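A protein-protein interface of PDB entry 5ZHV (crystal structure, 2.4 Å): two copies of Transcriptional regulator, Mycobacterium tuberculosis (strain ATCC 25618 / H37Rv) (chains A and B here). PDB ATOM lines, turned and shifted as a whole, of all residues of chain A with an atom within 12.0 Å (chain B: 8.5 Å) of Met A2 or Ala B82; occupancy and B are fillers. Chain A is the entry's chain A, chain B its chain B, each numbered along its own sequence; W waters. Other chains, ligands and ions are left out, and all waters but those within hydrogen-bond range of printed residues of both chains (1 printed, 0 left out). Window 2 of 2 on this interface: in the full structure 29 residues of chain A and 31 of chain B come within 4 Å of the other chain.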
ATOM      1  N   ALA A   1      -0.405  22.758  -3.448  1.00  0.00           N
ATOM      2  CA  ALA A   1       0.410  22.137  -2.350  1.00  0.00           C
ATOM      3  C   ALA A   1      -0.143  20.755  -1.928  1.00  0.00           C
ATOM      4  O   ALA A   1      -1.362  20.524  -1.937  1.00  0.00           O
ATOM      5  CB  ALA A   1       0.514  23.069  -1.159  1.00  0.00           C
ATOM      6  N   MET A   2       0.757  19.831  -1.595  1.00  0.00           N
ATOM      7  CA  MET A   2       0.355  18.538  -1.044  1.00  0.00           C
ATOM      8  C   MET A   2      -0.255  18.650   0.361  1.00  0.00           C
ATOM      9  O   MET A   2      -1.144  17.857   0.714  1.00  0.00           O
ATOM     10  CB  MET A   2       1.543  17.564  -1.013  1.00  0.00           C
ATOM     11  CG  MET A   2       2.049  17.111  -2.377  1.00  0.00           C
ATOM     12  SD  MET A   2       0.796  16.324  -3.419  1.00  0.00           S
ATOM     13  CE  MET A   2       0.338  14.886  -2.456  1.00  0.00           C
ATOM     14  N   ASP A   3       0.212  19.623   1.146  1.00  0.00           N
ATOM     15  CA  ASP A   3      -0.254  19.811   2.526  1.00  0.00           C
ATOM     16  C   ASP A   3      -0.701  21.272   2.744  1.00  0.00           C
ATOM     17  O   ASP A   3       0.055  22.080   3.343  1.00  0.00           O
ATOM     18  CB  ASP A   3       0.842  19.393   3.514  1.00  0.00           C
ATOM     19  CG  ASP A   3       0.371  19.338   4.955  1.00  0.00           C
ATOM     20  OD1 ASP A   3      -0.814  19.626   5.257  1.00  0.00           O
ATOM     21  OD2 ASP A   3       1.215  19.000   5.821  1.00  0.00           O
ATOM     22  N   PRO A   4      -1.933  21.604   2.284  1.00  0.00           N
ATOM     23  CA  PRO A   4      -2.428  22.982   2.298  1.00  0.00           C
ATOM     24  C   PRO A   4      -2.622  23.534   3.697  1.00  0.00           C
ATOM     25  O   PRO A   4      -2.413  24.734   3.903  1.00  0.00           O
ATOM     26  CB  PRO A   4      -3.757  22.905   1.545  1.00  0.00           C
ATOM     27  CG  PRO A   4      -3.744  21.568   0.851  1.00  0.00           C
ATOM     28  CD  PRO A   4      -2.933  20.671   1.741  1.00  0.00           C
ATOM     29  N   GLU A   5      -2.988  22.680   4.652  1.00  0.00           N
ATOM     30  CA  GLU A   5      -3.128  23.106   6.053  1.00  0.00           C
ATOM     31  C   GLU A   5      -1.771  23.510   6.653  1.00  0.00           C
ATOM     32  O   GLU A   5      -1.674  24.557   7.309  1.00  0.00           O
ATOM     33  CB  GLU A   5      -3.849  22.040   6.902  1.00  0.00           C
ATOM     34  CG  GLU A   5      -4.280  22.493   8.310  1.00  0.00           C
ATOM     35  CD  GLU A   5      -5.193  23.729   8.319  1.00  0.00           C
ATOM     36  OE1 GLU A   5      -6.130  23.815   7.491  1.00  0.00           O
ATOM     37  OE2 GLU A   5      -4.991  24.643   9.157  1.00  0.00           O
ATOM     38  N   PHE A   6      -0.722  22.718   6.393  1.00  0.00           N
ATOM     39  CA  PHE A   6       0.626  23.123   6.781  1.00  0.00           C
ATOM     40  C   PHE A   6       0.992  24.447   6.140  1.00  0.00           C
ATOM     41  O   PHE A   6       1.439  25.354   6.852  1.00  0.00           O
ATOM     42  CB  PHE A   6       1.705  22.110   6.423  1.00  0.00           C
ATOM     43  CG  PHE A   6       3.101  22.591   6.750  1.00  0.00           C
ATOM     44  CD1 PHE A   6       3.834  23.332   5.819  1.00  0.00           C
ATOM     45  CD2 PHE A   6       3.670  22.346   8.012  1.00  0.00           C
ATOM     46  CE1 PHE A   6       5.113  23.797   6.123  1.00  0.00           C
ATOM     47  CE2 PHE A   6       4.932  22.816   8.327  1.00  0.00           C
ATOM     48  CZ  PHE A   6       5.665  23.539   7.382  1.00  0.00           C
ATOM     49  N   MET A   7       0.824  24.554   4.813  1.00  0.00           N
ATOM     50  CA  MET A   7       1.189  25.791   4.103  1.00  0.00           C
ATOM     51  C   MET A   7       0.457  27.019   4.639  1.00  0.00           C
ATOM     52  O   MET A   7       1.051  28.073   4.801  1.00  0.00           O
ATOM     53  CB  MET A   7       1.027  25.663   2.588  1.00  0.00           C
ATOM     54  CG  MET A   7       2.033  24.720   1.945  1.00  0.00           C
ATOM     55  SD  MET A   7       3.806  25.016   2.274  1.00  0.00           S
ATOM     56  CE  MET A   7       4.452  23.558   1.424  1.00  0.00           C
ATOM     57  N   ARG A   8      -0.823  26.839   4.951  1.00  0.00           N
ATOM     58  CA  ARG A   8      -1.676  27.885   5.496  1.00  0.00           C
ATOM     59  C   ARG A   8      -1.179  28.329   6.887  1.00  0.00           C
ATOM     60  O   ARG A   8      -0.877  29.491   7.086  1.00  0.00           O
ATOM     61  CB  ARG A   8      -3.104  27.352   5.522  1.00  0.00           C
ATOM     62  CG  ARG A   8      -4.201  28.313   5.962  1.00  0.00           C
ATOM     63  CD  ARG A   8      -5.545  27.576   5.964  1.00  0.00           C
ATOM     64  NE  ARG A   8      -5.892  27.132   4.603  1.00  0.00           N
ATOM     65  CZ  ARG A   8      -6.060  25.868   4.203  1.00  0.00           C
ATOM     66  NH1 ARG A   8      -5.960  24.860   5.070  1.00  0.00           N
ATOM     67  NH2 ARG A   8      -6.340  25.628   2.923  1.00  0.00           N
ATOM     68  N   GLU A   9      -1.068  27.383   7.821  1.00  0.00           N
ATOM     69  CA  GLU A   9      -0.484  27.638   9.142  1.00  0.00           C
ATOM     70  C   GLU A   9       0.923  28.260   9.053  1.00  0.00           C
ATOM     71  O   GLU A   9       1.191  29.272   9.704  1.00  0.00           O
ATOM     72  CB  GLU A   9      -0.422  26.347   9.971  1.00  0.00           C
ATOM     73  CG  GLU A   9      -1.766  25.708  10.329  1.00  0.00           C
ATOM     74  CD  GLU A   9      -1.641  24.248  10.795  1.00  0.00           C
ATOM     75  OE1 GLU A   9      -0.565  23.611  10.607  1.00  0.00           O
ATOM     76  OE2 GLU A   9      -2.638  23.710  11.355  1.00  0.00           O
ATOM     77  N   PHE A  10       1.799  27.670   8.230  1.00  0.00           N
ATOM     78  CA  PHE A  10       3.191  28.110   8.112  1.00  0.00           C
ATOM     79  C   PHE A  10       3.310  29.506   7.504  1.00  0.00           C
ATOM     80  O   PHE A  10       4.185  30.294   7.910  1.00  0.00           O
ATOM     81  CB  PHE A  10       3.989  27.122   7.281  1.00  0.00           C
ATOM     82  CG  PHE A  10       5.470  27.402   7.231  1.00  0.00           C
ATOM     83  CD1 PHE A  10       6.295  27.090   8.310  1.00  0.00           C
ATOM     84  CD2 PHE A  10       6.053  27.959   6.086  1.00  0.00           C
ATOM     85  CE1 PHE A  10       7.671  27.338   8.250  1.00  0.00           C
ATOM     86  CE2 PHE A  10       7.425  28.206   6.021  1.00  0.00           C
ATOM     87  CZ  PHE A  10       8.235  27.894   7.101  1.00  0.00           C
ATOM     88  N   ARG B  16       2.345  19.222  13.121  1.00  0.00           N
ATOM     89  CA  ARG B  16       1.978  18.602  11.861  1.00  0.00           C
ATOM     90  C   ARG B  16       3.208  18.029  11.154  1.00  0.00           C
ATOM     91  O   ARG B  16       3.235  16.851  10.799  1.00  0.00           O
ATOM     92  CB  ARG B  16       1.281  19.610  11.002  1.00  0.00           C
ATOM     93  CG  ARG B  16       0.708  19.022   9.744  1.00  0.00           C
ATOM     94  CD  ARG B  16      -0.137  20.055   9.045  1.00  0.00           C
ATOM     95  NE  ARG B  16      -1.032  19.396   8.100  1.00  0.00           N
ATOM     96  CZ  ARG B  16      -2.280  19.044   8.368  1.00  0.00           C
ATOM     97  NH1 ARG B  16      -2.801  19.319   9.555  1.00  0.00           N
ATOM     98  NH2 ARG B  16      -2.999  18.435   7.436  1.00  0.00           N
ATOM     99  N   LEU B  20       4.331  13.890  10.577  1.00  0.00           N
ATOM    100  CA  LEU B  20       4.705  13.368   9.274  1.00  0.00           C
ATOM    101  C   LEU B  20       6.125  12.860   9.225  1.00  0.00           C
ATOM    102  O   LEU B  20       6.403  11.909   8.521  1.00  0.00           O
ATOM    103  CB  LEU B  20       4.556  14.424   8.183  1.00  0.00           C
ATOM    104  CG  LEU B  20       3.152  14.716   7.715  1.00  0.00           C
ATOM    105  CD1 LEU B  20       3.214  15.970   6.874  1.00  0.00           C
ATOM    106  CD2 LEU B  20       2.642  13.564   6.896  1.00  0.00           C
ATOM    107  N   LEU B  56      -5.054  14.317   9.465  1.00  0.00           N
ATOM    108  CA  LEU B  56      -4.001  13.911   8.549  1.00  0.00           C
ATOM    109  C   LEU B  56      -4.353  12.680   7.704  1.00  0.00           C
ATOM    110  O   LEU B  56      -3.941  12.585   6.536  1.00  0.00           O
ATOM    111  CB  LEU B  56      -2.676  13.704   9.294  1.00  0.00           C
ATOM    112  CG  LEU B  56      -1.902  14.972   9.671  1.00  0.00           C
ATOM    113  CD1 LEU B  56      -0.928  14.694  10.802  1.00  0.00           C
ATOM    114  CD2 LEU B  56      -1.175  15.479   8.423  1.00  0.00           C
ATOM    115  N   ASP B  59      -6.889  13.922   5.214  1.00  0.00           N
ATOM    116  CA  ASP B  59      -6.127  14.655   4.202  1.00  0.00           C
ATOM    117  C   ASP B  59      -5.339  13.742   3.268  1.00  0.00           C
ATOM    118  O   ASP B  59      -4.687  14.236   2.339  1.00  0.00           O
ATOM    119  CB  ASP B  59      -5.189  15.691   4.861  1.00  0.00           C
ATOM    120  CG  ASP B  59      -5.957  16.859   5.475  1.00  0.00           C
ATOM    121  OD1 ASP B  59      -7.150  17.031   5.105  1.00  0.00           O
ATOM    122  OD2 ASP B  59      -5.383  17.589   6.325  1.00  0.00           O
ATOM    123  N   GLY B  60      -5.400  12.430   3.522  1.00  0.00           N
ATOM    124  CA  GLY B  60      -4.656  11.430   2.759  1.00  0.00           C
ATOM    125  C   GLY B  60      -3.162  11.388   3.036  1.00  0.00           C
ATOM    126  O   GLY B  60      -2.425  10.748   2.286  1.00  0.00           O
ATOM    127  N   LEU B  61      -2.693  12.070   4.085  1.00  0.00           N
ATOM    128  CA  LEU B  61      -1.228  12.165   4.326  1.00  0.00           C
ATOM    129  C   LEU B  61      -0.721  11.070   5.258  1.00  0.00           C
ATOM    130  O   LEU B  61       0.446  10.646   5.173  1.00  0.00           O
ATOM    131  CB  LEU B  61      -0.810  13.568   4.790  1.00  0.00           C
ATOM    132  CG  LEU B  61      -1.304  14.791   3.955  1.00  0.00           C
ATOM    133  CD1 LEU B  61      -0.784  16.103   4.547  1.00  0.00           C
ATOM    134  CD2 LEU B  61      -0.945  14.721   2.465  1.00  0.00           C
ATOM    135  N   LEU B  62      -1.613  10.596   6.130  1.00  0.00           N
ATOM    136  CA  LEU B  62      -1.374   9.380   6.905  1.00  0.00           C
ATOM    137  C   LEU B  62      -2.368   8.288   6.544  1.00  0.00           C
ATOM    138  O   LEU B  62      -3.430   8.563   6.022  1.00  0.00           O
ATOM    139  CB  LEU B  62      -1.484   9.666   8.409  1.00  0.00           C
ATOM    140  CG  LEU B  62      -0.527  10.635   9.107  1.00  0.00           C
ATOM    141  CD1 LEU B  62      -0.907  10.770  10.584  1.00  0.00           C
ATOM    142  CD2 LEU B  62       0.947  10.240   8.916  1.00  0.00           C
ATOM    143  N   ALA B  79       3.023   7.286   7.135  1.00  0.00           N
ATOM    144  CA  ALA B  79       2.901   8.212   5.995  1.00  0.00           C
ATOM    145  C   ALA B  79       2.483   7.454   4.726  1.00  0.00           C
ATOM    146  O   ALA B  79       2.920   6.327   4.499  1.00  0.00           O
ATOM    147  CB  ALA B  79       4.204   8.937   5.768  1.00  0.00           C
ATOM    148  N   THR B  80       1.605   8.068   3.945  1.00  0.00           N
ATOM    149  CA  THR B  80       1.229   7.574   2.620  1.00  0.00           C
ATOM    150  C   THR B  80       2.259   8.149   1.655  1.00  0.00           C
ATOM    151  O   THR B  80       3.029   9.019   2.063  1.00  0.00           O
ATOM    152  CB  THR B  80      -0.164   8.110   2.196  1.00  0.00           C
ATOM    153  OG1 THR B  80      -0.134   9.548   2.165  1.00  0.00           O
ATOM    154  CG2 THR B  80      -1.246   7.611   3.111  1.00  0.00           C
ATOM    155  N   PRO B  81       2.270   7.690   0.375  1.00  0.00           N
ATOM    156  CA  PRO B  81       3.091   8.401  -0.617  1.00  0.00           C
ATOM    157  C   PRO B  81       2.830   9.923  -0.662  1.00  0.00           C
ATOM    158  O   PRO B  81       3.795  10.716  -0.761  1.00  0.00           O
ATOM    159  CB  PRO B  81       2.691   7.723  -1.925  1.00  0.00           C
ATOM    160  CG  PRO B  81       2.432   6.306  -1.508  1.00  0.00           C
ATOM    161  CD  PRO B  81       1.870   6.352  -0.115  1.00  0.00           C
ATOM    162  N   ALA B  82       1.559  10.322  -0.547  1.00  0.00           N
ATOM    163  CA  ALA B  82       1.182  11.742  -0.469  1.00  0.00           C
ATOM    164  C   ALA B  82       1.810  12.434   0.758  1.00  0.00           C
ATOM    165  O   ALA B  82       2.250  13.601   0.686  1.00  0.00           O
ATOM    166  CB  ALA B  82      -0.341  11.888  -0.460  1.00  0.00           C
ATOM    167  N   GLY B  83       1.866  11.697   1.871  1.00  0.00           N
ATOM    168  CA  GLY B  83       2.510  12.176   3.081  1.00  0.00           C
ATOM    169  C   GLY B  83       3.991  12.415   2.928  1.00  0.00           C
ATOM    170  O   GLY B  83       4.486  13.435   3.387  1.00  0.00           O
ATOM    171  N   ARG B  84       4.702  11.504   2.266  1.00  0.00           N
ATOM    172  CA  ARG B  84       6.149  11.683   2.009  1.00  0.00           C
ATOM    173  C   ARG B  84       6.397  12.884   1.128  1.00  0.00           C
ATOM    174  O   ARG B  84       7.333  13.642   1.384  1.00  0.00           O
ATOM    175  CB  ARG B  84       6.770  10.439   1.382  1.00  0.00           C
ATOM    176  CG  ARG B  84       6.643   9.235   2.284  1.00  0.00           C
ATOM    177  CD  ARG B  84       7.073   7.921   1.644  1.00  0.00           C
ATOM    178  NE  ARG B  84       6.781   6.847   2.577  1.00  0.00           N
ATOM    179  CZ  ARG B  84       7.554   6.512   3.625  1.00  0.00           C
ATOM    180  NH1 ARG B  84       8.711   7.140   3.855  1.00  0.00           N
ATOM    181  NH2 ARG B  84       7.179   5.520   4.440  1.00  0.00           N
ATOM    182  N   ALA B  85       5.549  13.068   0.115  1.00  0.00           N
ATOM    183  CA  ALA B  85       5.641  14.241  -0.770  1.00  0.00           C
ATOM    184  C   ALA B  85       5.329  15.542  -0.018  1.00  0.00           C
ATOM    185  O   ALA B  85       6.067  16.529  -0.176  1.00  0.00           O
ATOM    186  CB  ALA B  85       4.772  14.086  -2.022  1.00  0.00           C
ATOM    187  N   ALA B  86       4.273  15.524   0.821  1.00  0.00           N
ATOM    188  CA  ALA B  86       3.943  16.656   1.702  1.00  0.00           C
ATOM    189  C   ALA B  86       5.115  17.008   2.603  1.00  0.00           C
ATOM    190  O   ALA B  86       5.492  18.185   2.726  1.00  0.00           O
ATOM    191  CB  ALA B  86       2.709  16.356   2.527  1.00  0.00           C
ATOM    192  N   LEU B  87       5.726  15.979   3.199  1.00  0.00           N
ATOM    193  CA  LEU B  87       6.891  16.176   4.060  1.00  0.00           C
ATOM    194  C   LEU B  87       8.016  16.880   3.324  1.00  0.00           C
ATOM    195  O   LEU B  87       8.591  17.821   3.873  1.00  0.00           O
ATOM    196  CB  LEU B  87       7.357  14.860   4.680  1.00  0.00           C
ATOM    197  CG  LEU B  87       8.543  14.810   5.661  1.00  0.00           C
ATOM    198  CD1 LEU B  87       8.335  15.593   6.954  1.00  0.00           C
ATOM    199  CD2 LEU B  87       8.801  13.359   5.982  1.00  0.00           C
ATOM    200  N   THR B  88       8.287  16.469   2.080  1.00  0.00           N
ATOM    201  CA  THR B  88       9.338  17.101   1.274  1.00  0.00           C
ATOM    202  C   THR B  88       9.008  18.577   1.054  1.00  0.00           C
ATOM    203  O   THR B  88       9.874  19.430   1.274  1.00  0.00           O
ATOM    204  CB  THR B  88       9.552  16.366  -0.077  1.00  0.00           C
ATOM    205  OG1 THR B  88       9.982  15.026   0.167  1.00  0.00           O
ATOM    206  CG2 THR B  88      10.599  17.078  -0.961  1.00  0.00           C
ATOM    207  N   GLU B  89       7.757  18.859   0.667  1.00  0.00           N
ATOM    208  CA  GLU B  89       7.306  20.220   0.392  1.00  0.00           C
ATOM    209  C   GLU B  89       7.337  21.103   1.638  1.00  0.00           C
ATOM    210  O   GLU B  89       7.856  22.238   1.600  1.00  0.00           O
ATOM    211  CB  GLU B  89       5.916  20.218  -0.241  1.00  0.00           C
ATOM    212  CG  GLU B  89       5.949  19.877  -1.728  1.00  0.00           C
ATOM    213  CD  GLU B  89       4.581  19.746  -2.390  1.00  0.00           C
ATOM    214  OE1 GLU B  89       3.528  20.168  -1.795  1.00  0.00           O
ATOM    215  OE2 GLU B  89       4.577  19.208  -3.530  1.00  0.00           O
ATOM    216  N   ASP B  90       6.792  20.580   2.738  1.00  0.00           N
ATOM    217  CA  ASP B  90       6.805  21.295   4.005  1.00  0.00           C
ATOM    218  C   ASP B  90       8.228  21.586   4.473  1.00  0.00           C
ATOM    219  O   ASP B  90       8.523  22.732   4.818  1.00  0.00           O
ATOM    220  CB  ASP B  90       6.030  20.540   5.088  1.00  0.00           C
ATOM    221  CG  ASP B  90       4.574  20.243   4.704  1.00  0.00           C
ATOM    222  OD1 ASP B  90       4.061  20.768   3.666  1.00  0.00           O
ATOM    223  OD2 ASP B  90       3.964  19.452   5.463  1.00  0.00           O
HETATM  224  O   HOH W   1      -3.384  19.761   4.515  1.00  0.00           O
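The side-chain carboxylate (OE1) of Glu B89 sits at hydrogen-bond distance from the backbone NH (N) of Met A2, at 2.8 Å. The guanidinium group (NE) of Arg B16 is in salt-bridge range of the side-chain carboxylate (OD1) of Asp A3, at 2.9 Å. The side-chain carboxylate (OD2) of Asp A3 sits close to the side-chain carboxylate (OD2) of Asp B90 (2.8 Å).
OD1 of Asp A3 lies within hydrogen-bond range of N of Phe A6 (3.3 Å). The guanidinium group of Arg A8 lies within salt-bridge range of the side-chain carboxylate of Glu A5 (2.6 Å). NH2 of Arg B16 is in salt-bridge range of OD2 of Asp B59 (2.8 Å). The backbone NH (N) of Leu B61 sits at hydrogen-bond distance from the backbone carbonyl oxygen (O) of Leu B56 (2.8 Å). The backbone carbonyl oxygen of Leu B61 lies within hydrogen-bond range of the backbone NH of Thr B80 (3.1 Å). The side-chain hydroxyl of Thr B80 sits close to the backbone NH of Ala B82.
Ala A1 touches Glu B89. CE of Met A2 touches CB of Ala B82, at 3.7 Å. CB of Met A2 touches CA of Ala B86, 3.7 Å away. OD2 of Asp A3 touches CD1 of Leu B20, at 3.8 Å. Asp A3 touches Leu B61 (CG to CD1, 3.5 Å). CB of Asp A3 touches CB of Ala B86 (3.7 Å). Glu A5 touches Arg B16 (CB to CZ, 3.7 Å). Arg B16 touches Phe A6. OD1 of Asp B90 touches CE of Met A7 (3.6 Å). OE1 of Glu A9 touches CD of Arg B16 (3.9 Å).
Of the printed residues of chain B, Met A2 touches Leu B61, Ala B82, Ala B86 and Glu B89. Ala A1 touches one residue of chain B. No residue of chain A comes within 4 Å of Gly B60. Of chain A, only Met A2 (3.6 Å) and Asp A3 (3.5 Å) come within 4 Å of Leu B61. No residue of chain A comes within 4 Å of Thr B80. No residue of chain A comes within 4 Å of Pro B81. No residue of chain A comes within 4 Å of Ala B85. Ala B86 touches two residues of chain A. Of the printed residues of chain B, Asp A3 touches Arg B16, Leu B20, Leu B61, Ala B86 and Asp B90. Printed residues of chain B within 4 Å of Met A7: Glu B89 (3.7 Å) and Asp B90 (3.6 Å). The nearest residue of chain B that does not touch Met A2 is Ala B85 (4.1 Å).
Along chain A the printed residues that touch a printed residue of chain B span positions 1 to 9. Among the printed residues, 16 pairs touch across the chains.
No position is printed for both chains.
Water W1 lies within hydrogen-bond range of OD1 of Asp A3, N of Glu A5, NH2 of Arg B16 and OD2 of Asp B59.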
